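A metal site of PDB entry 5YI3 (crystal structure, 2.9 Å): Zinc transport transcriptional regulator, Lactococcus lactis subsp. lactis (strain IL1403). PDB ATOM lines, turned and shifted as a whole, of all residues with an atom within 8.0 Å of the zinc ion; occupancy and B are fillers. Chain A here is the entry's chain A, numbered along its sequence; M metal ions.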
ATOM      1  N   HIS A  23       3.368   0.965  21.596  1.00  0.00           N
ATOM      2  CA  HIS A  23       4.440   1.456  22.462  1.00  0.00           C
ATOM      3  C   HIS A  23       3.934   2.438  23.497  1.00  0.00           C
ATOM      4  O   HIS A  23       4.437   3.565  23.608  1.00  0.00           O
ATOM      5  CB  HIS A  23       5.548   2.121  21.647  1.00  0.00           C
ATOM      6  CG  HIS A  23       6.344   1.164  20.816  1.00  0.00           C
ATOM      7  ND1 HIS A  23       5.951   0.777  19.542  1.00  0.00           N
ATOM      8  CD2 HIS A  23       7.511   0.523  21.059  1.00  0.00           C
ATOM      9  CE1 HIS A  23       6.841  -0.060  19.052  1.00  0.00           C
ATOM     10  NE2 HIS A  23       7.793  -0.238  19.945  1.00  0.00           N
ATOM     11  N   GLU A  24       2.944   2.013  24.259  1.00  0.00           N
ATOM     12  CA  GLU A  24       2.296   2.871  25.220  1.00  0.00           C
ATOM     13  C   GLU A  24       1.202   2.068  25.898  1.00  0.00           C
ATOM     14  O   GLU A  24       0.677   1.133  25.309  1.00  0.00           O
ATOM     15  CB  GLU A  24       1.693   4.099  24.531  1.00  0.00           C
ATOM     16  CG  GLU A  24       1.178   5.150  25.491  1.00  0.00           C
ATOM     17  CD  GLU A  24       0.652   6.382  24.788  1.00  0.00           C
ATOM     18  OE1 GLU A  24      -0.479   6.323  24.278  1.00  0.00           O
ATOM     19  OE2 GLU A  24       1.371   7.406  24.758  1.00  0.00           O
ATOM     20  N   ILE A  25       0.878   2.408  27.130  1.00  0.00           N
ATOM     21  CA  ILE A  25      -0.119   1.649  27.873  1.00  0.00           C
ATOM     22  C   ILE A  25      -1.264   2.541  28.340  1.00  0.00           C
ATOM     23  O   ILE A  25      -1.068   3.418  29.169  1.00  0.00           O
ATOM     24  CB  ILE A  25       0.509   0.926  29.083  1.00  0.00           C
ATOM     25  CG1 ILE A  25       1.916   0.433  28.750  1.00  0.00           C
ATOM     26  CG2 ILE A  25      -0.337  -0.251  29.507  1.00  0.00           C
ATOM     27  CD1 ILE A  25       1.933  -0.866  28.023  1.00  0.00           C
ATOM     28  N   LEU A  26      -2.456   2.322  27.811  1.00  0.00           N
ATOM     29  CA  LEU A  26      -3.659   3.003  28.276  1.00  0.00           C
ATOM     30  C   LEU A  26      -4.778   2.003  28.598  1.00  0.00           C
ATOM     31  O   LEU A  26      -4.736   0.847  28.149  1.00  0.00           O
ATOM     32  CB  LEU A  26      -4.120   4.001  27.214  1.00  0.00           C
ATOM     33  CG  LEU A  26      -3.092   5.047  26.808  1.00  0.00           C
ATOM     34  CD1 LEU A  26      -3.460   5.696  25.494  1.00  0.00           C
ATOM     35  CD2 LEU A  26      -2.899   6.102  27.890  1.00  0.00           C
ATOM     36  N   THR A  37      -2.706   5.209  14.616  1.00  0.00           N
ATOM     37  CA  THR A  37      -1.832   4.478  15.552  1.00  0.00           C
ATOM     38  C   THR A  37      -1.684   5.256  16.847  1.00  0.00           C
ATOM     39  O   THR A  37      -1.788   6.474  16.827  1.00  0.00           O
ATOM     40  CB  THR A  37      -0.391   4.276  15.014  1.00  0.00           C
ATOM     41  OG1 THR A  37       0.323   5.523  14.997  1.00  0.00           O
ATOM     42  CG2 THR A  37      -0.399   3.651  13.626  1.00  0.00           C
ATOM     43  N   SER A  38      -1.414   4.576  17.953  1.00  0.00           N
ATOM     44  CA  SER A  38      -1.268   5.298  19.216  1.00  0.00           C
ATOM     45  C   SER A  38      -0.221   6.402  19.050  1.00  0.00           C
ATOM     46  O   SER A  38      -0.489   7.577  19.315  1.00  0.00           O
ATOM     47  CB  SER A  38      -0.936   4.338  20.365  1.00  0.00           C
ATOM     48  OG  SER A  38       0.369   3.819  20.207  1.00  0.00           O
ATOM     49  N   THR A  39       0.960   6.041  18.563  1.00  0.00           N
ATOM     50  CA  THR A  39       2.019   7.007  18.305  1.00  0.00           C
ATOM     51  C   THR A  39       1.580   8.204  17.450  1.00  0.00           C
ATOM     52  O   THR A  39       2.065   9.315  17.610  1.00  0.00           O
ATOM     53  CB  THR A  39       3.223   6.342  17.653  1.00  0.00           C
ATOM     54  OG1 THR A  39       3.902   5.544  18.633  1.00  0.00           O
ATOM     55  CG2 THR A  39       4.177   7.408  17.090  1.00  0.00           C
ATOM     56  N   GLN A  40       0.663   7.974  16.528  1.00  0.00           N
ATOM     57  CA  GLN A  40       0.121   9.070  15.736  1.00  0.00           C
ATOM     58  C   GLN A  40      -0.852   9.924  16.552  1.00  0.00           C
ATOM     59  O   GLN A  40      -0.951  11.135  16.343  1.00  0.00           O
ATOM     60  CB  GLN A  40      -0.523   8.557  14.450  1.00  0.00           C
ATOM     61  CG  GLN A  40       0.459   8.376  13.328  1.00  0.00           C
ATOM     62  CD  GLN A  40       0.275   7.082  12.593  1.00  0.00           C
ATOM     63  OE1 GLN A  40      -0.813   6.520  12.565  1.00  0.00           O
ATOM     64  NE2 GLN A  40       1.358   6.594  11.981  1.00  0.00           N
ATOM     65  N   GLU A  41      -1.555   9.305  17.486  1.00  0.00           N
ATOM     66  CA  GLU A  41      -2.439  10.054  18.363  1.00  0.00           C
ATOM     67  C   GLU A  41      -1.584  10.927  19.254  1.00  0.00           C
ATOM     68  O   GLU A  41      -1.751  12.142  19.317  1.00  0.00           O
ATOM     69  CB  GLU A  41      -3.259   9.096  19.247  1.00  0.00           C
ATOM     70  CG  GLU A  41      -4.314   8.288  18.486  1.00  0.00           C
ATOM     71  CD  GLU A  41      -5.125   7.348  19.380  1.00  0.00           C
ATOM     72  OE1 GLU A  41      -4.974   7.404  20.628  1.00  0.00           O
ATOM     73  OE2 GLU A  41      -5.904   6.550  18.827  1.00  0.00           O
ATOM     74  N   HIS A  42      -0.654  10.275  19.933  1.00  0.00           N
ATOM     75  CA  HIS A  42       0.169  10.928  20.919  1.00  0.00           C
ATOM     76  C   HIS A  42       0.856  12.148  20.321  1.00  0.00           C
ATOM     77  O   HIS A  42       1.028  13.169  21.003  1.00  0.00           O
ATOM     78  CB  HIS A  42       1.215   9.954  21.451  1.00  0.00           C
ATOM     79  CG  HIS A  42       1.801  10.380  22.747  1.00  0.00           C
ATOM     80  ND1 HIS A  42       1.328   9.945  23.970  1.00  0.00           N
ATOM     81  CD2 HIS A  42       2.819  11.235  23.029  1.00  0.00           C
ATOM     82  CE1 HIS A  42       2.024  10.496  24.939  1.00  0.00           C
ATOM     83  NE2 HIS A  42       2.939  11.277  24.398  1.00  0.00           N
ATOM     84  N   ILE A  43       1.255  12.025  19.059  1.00  0.00           N
ATOM     85  CA  ILE A  43       1.917  13.147  18.395  1.00  0.00           C
ATOM     86  C   ILE A  43       0.955  14.305  18.253  1.00  0.00           C
ATOM     87  O   ILE A  43       1.344  15.468  18.333  1.00  0.00           O
ATOM     88  CB  ILE A  43       2.414  12.793  17.005  1.00  0.00           C
ATOM     89  CG1 ILE A  43       3.517  11.752  17.090  1.00  0.00           C
ATOM     90  CG2 ILE A  43       2.943  14.029  16.323  1.00  0.00           C
ATOM     91  CD1 ILE A  43       4.094  11.425  15.747  1.00  0.00           C
ATOM     92  N   MET A  45      -1.499  14.940  20.291  1.00  0.00           N
ATOM     93  CA  MET A  45      -1.664  15.479  21.617  1.00  0.00           C
ATOM     94  C   MET A  45      -0.524  16.433  21.937  1.00  0.00           C
ATOM     95  O   MET A  45      -0.697  17.422  22.633  1.00  0.00           O
ATOM     96  CB  MET A  45      -1.689  14.369  22.643  1.00  0.00           C
ATOM     97  CG  MET A  45      -2.139  14.819  23.993  1.00  0.00           C
ATOM     98  SD  MET A  45      -1.616  13.583  25.168  1.00  0.00           S
ATOM     99  CE  MET A  45       0.155  13.707  24.972  1.00  0.00           C
ATOM    100  N   LEU A  46       0.649  16.126  21.401  1.00  0.00           N
ATOM    101  CA  LEU A  46       1.798  16.967  21.655  1.00  0.00           C
ATOM    102  C   LEU A  46       1.666  18.275  20.892  1.00  0.00           C
ATOM    103  O   LEU A  46       2.030  19.343  21.393  1.00  0.00           O
ATOM    104  CB  LEU A  46       3.084  16.229  21.281  1.00  0.00           C
ATOM    105  CG  LEU A  46       3.365  15.001  22.151  1.00  0.00           C
ATOM    106  CD1 LEU A  46       4.701  14.383  21.796  1.00  0.00           C
ATOM    107  CD2 LEU A  46       3.328  15.353  23.627  1.00  0.00           C
ATOM    108  N   LEU A  61       9.044  11.262  22.165  1.00  0.00           N
ATOM    109  CA  LEU A  61       8.612   9.875  21.957  1.00  0.00           C
ATOM    110  C   LEU A  61       9.723   8.833  21.937  1.00  0.00           C
ATOM    111  O   LEU A  61       9.454   7.652  21.724  1.00  0.00           O
ATOM    112  CB  LEU A  61       7.886   9.749  20.622  1.00  0.00           C
ATOM    113  CG  LEU A  61       6.382   9.991  20.585  1.00  0.00           C
ATOM    114  CD1 LEU A  61       6.001  11.175  21.475  1.00  0.00           C
ATOM    115  CD2 LEU A  61       5.926  10.191  19.133  1.00  0.00           C
ATOM    116  N   HIS A 108      -7.485  11.861  23.081  1.00  0.00           N
ATOM    117  CA  HIS A 108      -6.288  11.177  23.551  1.00  0.00           C
ATOM    118  C   HIS A 108      -5.799  11.748  24.880  1.00  0.00           C
ATOM    119  O   HIS A 108      -5.444  11.000  25.791  1.00  0.00           O
ATOM    120  CB  HIS A 108      -5.168  11.213  22.511  1.00  0.00           C
ATOM    121  CG  HIS A 108      -4.047  10.261  22.809  1.00  0.00           C
ATOM    122  ND1 HIS A 108      -4.247   8.903  22.974  1.00  0.00           N
ATOM    123  CD2 HIS A 108      -2.721  10.460  22.971  1.00  0.00           C
ATOM    124  CE1 HIS A 108      -3.086   8.317  23.237  1.00  0.00           C
ATOM    125  NE2 HIS A 108      -2.145   9.243  23.229  1.00  0.00           N
ATOM    126  N   ALA A 109      -5.794  13.062  24.978  1.00  0.00           N
ATOM    127  CA  ALA A 109      -5.434  13.739  26.214  1.00  0.00           C
ATOM    128  C   ALA A 109      -6.172  13.121  27.404  1.00  0.00           C
ATOM    129  O   ALA A 109      -5.559  12.531  28.310  1.00  0.00           O
ATOM    130  CB  ALA A 109      -5.751  15.219  26.115  1.00  0.00           C
ATOM    131  N   HIS A 111      -7.881  10.470  27.550  1.00  0.00           N
ATOM    132  CA  HIS A 111      -7.657   9.035  27.611  1.00  0.00           C
ATOM    133  C   HIS A 111      -6.413   8.720  28.430  1.00  0.00           C
ATOM    134  O   HIS A 111      -6.313   7.670  29.067  1.00  0.00           O
ATOM    135  CB  HIS A 111      -7.539   8.474  26.206  1.00  0.00           C
ATOM    136  CG  HIS A 111      -7.391   6.988  26.149  1.00  0.00           C
ATOM    137  ND1 HIS A 111      -7.376   6.283  24.968  1.00  0.00           N
ATOM    138  CD2 HIS A 111      -7.259   6.069  27.138  1.00  0.00           C
ATOM    139  CE1 HIS A 111      -7.243   4.999  25.225  1.00  0.00           C
ATOM    140  NE2 HIS A 111      -7.156   4.840  26.539  1.00  0.00           N
ATOM    141  N   HIS A 112      -5.445   9.626  28.420  1.00  0.00           N
ATOM    142  CA  HIS A 112      -4.249   9.478  29.234  1.00  0.00           C
ATOM    143  C   HIS A 112      -4.590   9.727  30.704  1.00  0.00           C
ATOM    144  O   HIS A 112      -4.019   9.093  31.599  1.00  0.00           O
ATOM    145  CB  HIS A 112      -3.164  10.449  28.770  1.00  0.00           C
ATOM    146  CG  HIS A 112      -2.051   9.814  27.991  1.00  0.00           C
ATOM    147  ND1 HIS A 112      -0.853   9.466  28.562  1.00  0.00           N
ATOM    148  CD2 HIS A 112      -1.955   9.497  26.681  1.00  0.00           C
ATOM    149  CE1 HIS A 112      -0.067   8.942  27.636  1.00  0.00           C
ATOM    150  NE2 HIS A 112      -0.716   8.945  26.486  1.00  0.00           N
HETATM  151 ZN    ZN M   1      -0.307   8.752  24.200  1.00  0.00          ZN
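A ring nitrogen (ND1) of His 108 is in hydrogen-bond range of the side-chain carboxylate (OE1) of Glu 41 (2.9 Å).
Within 4 Å of the zinc ion: Glu 24, His 42, His 108 and His 112. The nearest printed residue that does not touch the zinc ion is Leu 26 (4.6 Å).
ND1 of His 42 binds the zinc ion, at 2.0 Å. The zinc ion is bound by NE2 of His 108, 2.1 Å away. The side-chain carboxylate (OE2) of Glu 24 is bound to the zinc ion (2.2 Å). The zinc ion is bound by NE2 of His 112, 2.3 Å away. OE1 of Glu 24 binds the zinc ion, 2.4 Å away.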
